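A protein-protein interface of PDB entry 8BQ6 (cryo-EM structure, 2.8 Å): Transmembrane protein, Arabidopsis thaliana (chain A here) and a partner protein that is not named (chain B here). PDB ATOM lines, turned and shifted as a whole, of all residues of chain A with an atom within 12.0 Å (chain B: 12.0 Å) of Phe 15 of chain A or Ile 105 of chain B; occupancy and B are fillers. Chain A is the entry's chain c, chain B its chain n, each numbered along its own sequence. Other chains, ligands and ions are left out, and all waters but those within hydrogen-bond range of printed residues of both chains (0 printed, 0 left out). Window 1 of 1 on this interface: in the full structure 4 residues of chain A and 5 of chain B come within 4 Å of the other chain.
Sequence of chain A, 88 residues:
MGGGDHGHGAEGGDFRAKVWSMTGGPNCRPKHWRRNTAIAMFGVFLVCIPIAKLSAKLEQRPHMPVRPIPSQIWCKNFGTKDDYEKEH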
ATOM      1  N   GLY A  13      32.645  12.677  14.693  1.00  0.00           N
ATOM      2  CA  GLY A  13      33.084  11.826  13.605  1.00  0.00           C
ATOM      3  C   GLY A  13      32.033  11.719  12.522  1.00  0.00           C
ATOM      4  O   GLY A  13      31.748  12.690  11.822  1.00  0.00           O
ATOM      5  N   ASP A  14      31.446  10.533  12.384  1.00  0.00           N
ATOM      6  CA  ASP A  14      30.411  10.300  11.390  1.00  0.00           C
ATOM      7  C   ASP A  14      29.010  10.367  11.977  1.00  0.00           C
ATOM      8  O   ASP A  14      28.156  11.087  11.451  1.00  0.00           O
ATOM      9  CB  ASP A  14      30.626   8.940  10.710  1.00  0.00           C
ATOM     10  CG  ASP A  14      29.632   8.682   9.592  1.00  0.00           C
ATOM     11  OD1 ASP A  14      28.785   9.561   9.329  1.00  0.00           O
ATOM     12  OD2 ASP A  14      29.704   7.599   8.973  1.00  0.00           O
ATOM     13  N   PHE A  15      28.743   9.630  13.057  1.00  0.00           N
ATOM     14  CA  PHE A  15      27.390   9.623  13.599  1.00  0.00           C
ATOM     15  C   PHE A  15      27.132  10.803  14.525  1.00  0.00           C
ATOM     16  O   PHE A  15      25.972  11.151  14.765  1.00  0.00           O
ATOM     17  CB  PHE A  15      27.104   8.301  14.320  1.00  0.00           C
ATOM     18  CG  PHE A  15      27.811   8.143  15.642  1.00  0.00           C
ATOM     19  CD1 PHE A  15      27.272   8.668  16.805  1.00  0.00           C
ATOM     20  CD2 PHE A  15      28.990   7.426  15.726  1.00  0.00           C
ATOM     21  CE1 PHE A  15      27.910   8.512  18.013  1.00  0.00           C
ATOM     22  CE2 PHE A  15      29.630   7.264  16.936  1.00  0.00           C
ATOM     23  CZ  PHE A  15      29.088   7.807  18.080  1.00  0.00           C
ATOM     24  N   ARG A  16      28.185  11.425  15.056  1.00  0.00           N
ATOM     25  CA  ARG A  16      27.981  12.532  15.979  1.00  0.00           C
ATOM     26  C   ARG A  16      27.420  13.765  15.286  1.00  0.00           C
ATOM     27  O   ARG A  16      26.910  14.662  15.964  1.00  0.00           O
ATOM     28  CB  ARG A  16      29.290  12.851  16.693  1.00  0.00           C
ATOM     29  CG  ARG A  16      30.008  11.598  17.154  1.00  0.00           C
ATOM     30  CD  ARG A  16      30.588  11.772  18.536  1.00  0.00           C
ATOM     31  NE  ARG A  16      31.773  12.616  18.511  1.00  0.00           N
ATOM     32  CZ  ARG A  16      33.014  12.162  18.428  1.00  0.00           C
ATOM     33  NH1 ARG A  16      33.276  10.868  18.420  1.00  0.00           N
ATOM     34  NH2 ARG A  16      34.019  13.030  18.358  1.00  0.00           N
ATOM     35  N   ALA A  17      27.482  13.819  13.957  1.00  0.00           N
ATOM     36  CA  ALA A  17      26.861  14.909  13.217  1.00  0.00           C
ATOM     37  C   ALA A  17      25.340  14.833  13.223  1.00  0.00           C
ATOM     38  O   ALA A  17      24.689  15.817  12.858  1.00  0.00           O
ATOM     39  CB  ALA A  17      27.373  14.918  11.779  1.00  0.00           C
ATOM     40  N   LYS A  18      24.763  13.697  13.608  1.00  0.00           N
ATOM     41  CA  LYS A  18      23.320  13.538  13.714  1.00  0.00           C
ATOM     42  C   LYS A  18      22.826  13.605  15.149  1.00  0.00           C
ATOM     43  O   LYS A  18      21.657  13.304  15.407  1.00  0.00           O
ATOM     44  CB  LYS A  18      22.886  12.213  13.096  1.00  0.00           C
ATOM     45  CG  LYS A  18      23.480  11.935  11.738  1.00  0.00           C
ATOM     46  CD  LYS A  18      23.073  10.559  11.244  1.00  0.00           C
ATOM     47  CE  LYS A  18      21.648  10.215  11.655  1.00  0.00           C
ATOM     48  NZ  LYS A  18      20.649  11.125  11.039  1.00  0.00           N
ATOM     49  N   VAL A  19      23.687  13.978  16.088  1.00  0.00           N
ATOM     50  CA  VAL A  19      23.362  13.959  17.505  1.00  0.00           C
ATOM     51  C   VAL A  19      23.287  15.398  17.991  1.00  0.00           C
ATOM     52  O   VAL A  19      24.261  16.153  17.880  1.00  0.00           O
ATOM     53  CB  VAL A  19      24.392  13.149  18.305  1.00  0.00           C
ATOM     54  CG1 VAL A  19      24.275  13.451  19.782  1.00  0.00           C
ATOM     55  CG2 VAL A  19      24.211  11.664  18.036  1.00  0.00           C
ATOM     56  N   TRP A  20      22.129  15.776  18.521  1.00  0.00           N
ATOM     57  CA  TRP A  20      21.914  17.108  19.061  1.00  0.00           C
ATOM     58  C   TRP A  20      22.381  17.162  20.512  1.00  0.00           C
ATOM     59  O   TRP A  20      22.142  16.225  21.280  1.00  0.00           O
ATOM     60  CB  TRP A  20      20.436  17.483  18.961  1.00  0.00           C
ATOM     61  CG  TRP A  20      20.168  18.926  19.197  1.00  0.00           C
ATOM     62  CD1 TRP A  20      20.060  19.892  18.252  1.00  0.00           C
ATOM     63  CD2 TRP A  20      19.955  19.569  20.458  1.00  0.00           C
ATOM     64  NE1 TRP A  20      19.811  21.106  18.840  1.00  0.00           N
ATOM     65  CE2 TRP A  20      19.736  20.934  20.197  1.00  0.00           C
ATOM     66  CE3 TRP A  20      19.935  19.126  21.783  1.00  0.00           C
ATOM     67  CZ2 TRP A  20      19.499  21.858  21.208  1.00  0.00           C
ATOM     68  CZ3 TRP A  20      19.696  20.044  22.785  1.00  0.00           C
ATOM     69  CH2 TRP A  20      19.483  21.396  22.493  1.00  0.00           C
ATOM     70  N   SER A  21      23.046  18.255  20.878  1.00  0.00           N
ATOM     71  CA  SER A  21      23.483  18.476  22.249  1.00  0.00           C
ATOM     72  C   SER A  21      23.521  19.971  22.530  1.00  0.00           C
ATOM     73  O   SER A  21      23.727  20.789  21.632  1.00  0.00           O
ATOM     74  CB  SER A  21      24.860  17.860  22.519  1.00  0.00           C
ATOM     75  OG  SER A  21      25.813  18.325  21.582  1.00  0.00           O
ATOM     76  N   GLY A  24      26.973  21.525  21.904  1.00  0.00           N
ATOM     77  CA  GLY A  24      27.352  21.560  20.509  1.00  0.00           C
ATOM     78  C   GLY A  24      28.109  20.353  20.000  1.00  0.00           C
ATOM     79  O   GLY A  24      28.341  20.262  18.788  1.00  0.00           O
ATOM     80  N   GLY A  25      28.500  19.429  20.869  1.00  0.00           N
ATOM     81  CA  GLY A  25      29.217  18.256  20.436  1.00  0.00           C
ATOM     82  C   GLY A  25      30.652  18.573  20.071  1.00  0.00           C
ATOM     83  O   GLY A  25      31.212  19.590  20.486  1.00  0.00           O
ATOM     84  N   PRO A  26      31.272  17.713  19.269  1.00  0.00           N
ATOM     85  CA  PRO A  26      32.706  17.855  19.000  1.00  0.00           C
ATOM     86  C   PRO A  26      32.998  18.767  17.819  1.00  0.00           C
ATOM     87  O   PRO A  26      32.376  18.665  16.757  1.00  0.00           O
ATOM     88  CB  PRO A  26      33.146  16.418  18.706  1.00  0.00           C
ATOM     89  CG  PRO A  26      31.897  15.717  18.252  1.00  0.00           C
ATOM     90  CD  PRO A  26      30.696  16.563  18.557  1.00  0.00           C
ATOM     91  N   ASN A  27      33.979  19.651  18.015  1.00  0.00           N
ATOM     92  CA  ASN A  27      34.430  20.592  16.988  1.00  0.00           C
ATOM     93  C   ASN A  27      33.278  21.465  16.499  1.00  0.00           C
ATOM     94  O   ASN A  27      33.030  21.597  15.299  1.00  0.00           O
ATOM     95  CB  ASN A  27      35.090  19.864  15.817  1.00  0.00           C
ATOM     96  CG  ASN A  27      36.278  19.046  16.242  1.00  0.00           C
ATOM     97  OD1 ASN A  27      37.221  19.565  16.839  1.00  0.00           O
ATOM     98  ND2 ASN A  27      36.247  17.755  15.935  1.00  0.00           N
ATOM     99  N   ASN B  98      40.151  10.957  23.449  1.00  0.00           N
ATOM    100  CA  ASN B  98      39.507  11.351  22.200  1.00  0.00           C
ATOM    101  C   ASN B  98      39.659  10.285  21.122  1.00  0.00           C
ATOM    102  O   ASN B  98      40.208  10.563  20.049  1.00  0.00           O
ATOM    103  CB  ASN B  98      40.071  12.682  21.709  1.00  0.00           C
ATOM    104  CG  ASN B  98      39.832  13.797  22.691  1.00  0.00           C
ATOM    105  OD1 ASN B  98      38.765  13.881  23.296  1.00  0.00           O
ATOM    106  ND2 ASN B  98      40.825  14.656  22.868  1.00  0.00           N
ATOM    107  N   PRO B  99      39.194   9.062  21.361  1.00  0.00           N
ATOM    108  CA  PRO B  99      39.315   8.026  20.334  1.00  0.00           C
ATOM    109  C   PRO B  99      38.309   8.234  19.213  1.00  0.00           C
ATOM    110  O   PRO B  99      37.297   8.921  19.372  1.00  0.00           O
ATOM    111  CB  PRO B  99      39.035   6.737  21.108  1.00  0.00           C
ATOM    112  CG  PRO B  99      38.116   7.164  22.196  1.00  0.00           C
ATOM    113  CD  PRO B  99      38.462   8.580  22.546  1.00  0.00           C
ATOM    114  N   THR B 100      38.608   7.638  18.064  1.00  0.00           N
ATOM    115  CA  THR B 100      37.736   7.789  16.910  1.00  0.00           C
ATOM    116  C   THR B 100      36.422   7.050  17.150  1.00  0.00           C
ATOM    117  O   THR B 100      36.403   6.019  17.832  1.00  0.00           O
ATOM    118  CB  THR B 100      38.410   7.266  15.638  1.00  0.00           C
ATOM    119  OG1 THR B 100      38.859   5.921  15.841  1.00  0.00           O
ATOM    120  CG2 THR B 100      39.591   8.146  15.254  1.00  0.00           C
ATOM    121  N   PRO B 101      35.306   7.552  16.618  1.00  0.00           N
ATOM    122  CA  PRO B 101      34.027   6.895  16.863  1.00  0.00           C
ATOM    123  C   PRO B 101      34.007   5.509  16.249  1.00  0.00           C
ATOM    124  O   PRO B 101      34.632   5.268  15.201  1.00  0.00           O
ATOM    125  CB  PRO B 101      33.013   7.823  16.170  1.00  0.00           C
ATOM    126  CG  PRO B 101      33.728   9.086  15.927  1.00  0.00           C
ATOM    127  CD  PRO B 101      35.168   8.767  15.804  1.00  0.00           C
ATOM    128  N   PRO B 102      33.312   4.560  16.866  1.00  0.00           N
ATOM    129  CA  PRO B 102      33.119   3.261  16.217  1.00  0.00           C
ATOM    130  C   PRO B 102      32.188   3.390  15.023  1.00  0.00           C
ATOM    131  O   PRO B 102      31.336   4.277  14.961  1.00  0.00           O
ATOM    132  CB  PRO B 102      32.499   2.397  17.320  1.00  0.00           C
ATOM    133  CG  PRO B 102      31.878   3.355  18.259  1.00  0.00           C
ATOM    134  CD  PRO B 102      32.637   4.646  18.172  1.00  0.00           C
ATOM    135  N   ALA B 103      32.370   2.494  14.059  1.00  0.00           N
ATOM    136  CA  ALA B 103      31.492   2.436  12.902  1.00  0.00           C
ATOM    137  C   ALA B 103      30.318   1.504  13.178  1.00  0.00           C
ATOM    138  O   ALA B 103      30.397   0.588  14.000  1.00  0.00           O
ATOM    139  CB  ALA B 103      32.252   1.968  11.660  1.00  0.00           C
ATOM    140  N   GLY B 104      29.219   1.744  12.467  1.00  0.00           N
ATOM    141  CA  GLY B 104      28.025   0.942  12.636  1.00  0.00           C
ATOM    142  C   GLY B 104      26.990   1.532  13.560  1.00  0.00           C
ATOM    143  O   GLY B 104      26.038   0.834  13.927  1.00  0.00           O
ATOM    144  N   ILE B 105      27.146   2.792  13.950  1.00  0.00           N
ATOM    145  CA  ILE B 105      26.237   3.467  14.865  1.00  0.00           C
ATOM    146  C   ILE B 105      25.192   4.192  14.029  1.00  0.00           C
ATOM    147  O   ILE B 105      25.535   4.926  13.095  1.00  0.00           O
ATOM    148  CB  ILE B 105      26.988   4.453  15.775  1.00  0.00           C
ATOM    149  CG1 ILE B 105      28.094   3.755  16.577  1.00  0.00           C
ATOM    150  CG2 ILE B 105      26.022   5.143  16.713  1.00  0.00           C
ATOM    151  CD1 ILE B 105      27.672   2.502  17.294  1.00  0.00           C
ATOM    152  N   GLU B 106      23.919   3.922  14.331  1.00  0.00           N
ATOM    153  CA  GLU B 106      22.806   4.587  13.612  1.00  0.00           C
ATOM    154  C   GLU B 106      21.964   5.386  14.602  1.00  0.00           C
ATOM    155  O   GLU B 106      21.820   4.938  15.744  1.00  0.00           O
ATOM    156  CB  GLU B 106      21.937   3.559  12.886  1.00  0.00           C
ATOM    157  CG  GLU B 106      22.651   2.820  11.771  1.00  0.00           C
ATOM    158  CD  GLU B 106      22.773   1.328  12.020  1.00  0.00           C
ATOM    159  OE1 GLU B 106      22.520   0.548  11.084  1.00  0.00           O
ATOM    160  OE2 GLU B 106      23.111   0.952  13.153  1.00  0.00           O
ATOM    161  N   ILE B 107      21.427   6.519  14.172  1.00  0.00           N
ATOM    162  CA  ILE B 107      20.625   7.410  15.002  1.00  0.00           C
ATOM    163  C   ILE B 107      19.220   7.460  14.423  1.00  0.00           C
ATOM    164  O   ILE B 107      19.038   7.789  13.245  1.00  0.00           O
ATOM    165  CB  ILE B 107      21.242   8.818  15.072  1.00  0.00           C
ATOM    166  CG1 ILE B 107      22.615   8.778  15.742  1.00  0.00           C
ATOM    167  CG2 ILE B 107      20.334   9.753  15.832  1.00  0.00           C
ATOM    168  CD1 ILE B 107      22.634   8.076  17.076  1.00  0.00           C
ATOM    169  N   VAL B 108      18.246   7.096  15.260  1.00  0.00           N
ATOM    170  CA  VAL B 108      16.824   7.044  14.823  1.00  0.00           C
ATOM    171  C   VAL B 108      16.116   8.357  15.148  1.00  0.00           C
ATOM    172  O   VAL B 108      16.232   8.825  16.293  1.00  0.00           O
ATOM    173  CB  VAL B 108      16.101   5.849  15.477  1.00  0.00           C
ATOM    174  CG1 VAL B 108      14.669   5.691  14.993  1.00  0.00           C
ATOM    175  CG2 VAL B 108      16.876   4.552  15.314  1.00  0.00           C
ATOM    176  N   TYR B 109      15.436   8.940  14.168  1.00  0.00           N
ATOM    177  CA  TYR B 109      14.642  10.146  14.337  1.00  0.00           C
ATOM    178  C   TYR B 109      13.169   9.780  14.447  1.00  0.00           C
ATOM    179  O   TYR B 109      12.734   8.738  13.949  1.00  0.00           O
ATOM    180  CB  TYR B 109      14.839  11.111  13.167  1.00  0.00           C
ATOM    181  CG  TYR B 109      16.195  11.766  13.136  1.00  0.00           C
ATOM    182  CD1 TYR B 109      16.923  11.947  14.301  1.00  0.00           C
ATOM    183  CD2 TYR B 109      16.744  12.212  11.945  1.00  0.00           C
ATOM    184  CE1 TYR B 109      18.159  12.545  14.280  1.00  0.00           C
ATOM    185  CE2 TYR B 109      17.982  12.817  11.915  1.00  0.00           C
ATOM    186  CZ  TYR B 109      18.685  12.980  13.086  1.00  0.00           C
ATOM    187  OH  TYR B 109      19.920  13.581  13.064  1.00  0.00           O
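Of the 13 printed residues of chain A, 4 touch a printed residue of chain B.
Hydrophobic or aromatic side chains of chain A that line the printed part of chain B: Phe 15.
Printed residues of chain B that touch a printed residue of chain A: Pro 101, Pro 102, Ile 105, Ile 107 and Tyr 109.
Hydrophobic or aromatic side chains of chain B that line the printed part of chain A: Pro 101, Ile 105, Ile 107 and Tyr 109.
Among the printed residues, 7 pairs touch across the chains.
Phe 15 of chain A touches just these residues of chain B: Pro 101 (3.5 Å), Pro 102 (3.97 Å) and Ile 105 (3.6 Å).
Of chain A, only Phe 15 comes within 4 Å of Ile 105 of chain B.
Printed residues of chain B within 4 Å of Gly 13 of chain A: Pro 101 (3.6 Å).
No residue of chain B comes within 4 Å of Asp 14 of chain A.
Of the printed residues of chain B, Arg 16 of chain A touches Pro 101 (3.1 Å).
No residue of chain B comes within 4 Å of Ala 17 of chain A.
Pro 102 of chain B touches just one residue of chain A: Phe 15.
No residue of chain A comes within 4 Å of Ala 103 of chain B.
No residue of chain A comes within 4 Å of Gly 104 of chain B.
Of the printed residues of chain A, Ile 107 of chain B touches Lys 18.
Of the printed residues of chain A, Tyr 109 of chain B touches Lys 18.
Asn 27 of chain A touches none of the printed residues of chain B.
Thr 100 of chain B touches none of the printed residues of chain A.
The nearest printed residue of chain A that does not touch Tyr 109 of chain B is Val 19 of chain A (4.8 Å).
Gly 13 of chain A touches Pro 101 of chain B (CA to CG, 3.6 Å).
Phe 15 of chain A touches Pro 101 of chain B (CE2 to CB, 3.5 Å).
Pro 102 of chain B touches Phe 15 of chain A.
Phe 15 of chain A touches Ile 105 of chain B.
Arg 16 of chain A touches Pro 101 of chain B.
Ile 107 of chain B touches Lys 18 of chain A (CB to CE, 3.7 Å).
The backbone carbonyl oxygen (O) of Lys 18 of chain A is in hydrogen-bond range of the side-chain hydroxyl (OH) of Tyr 109 of chain B (2.9 Å).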
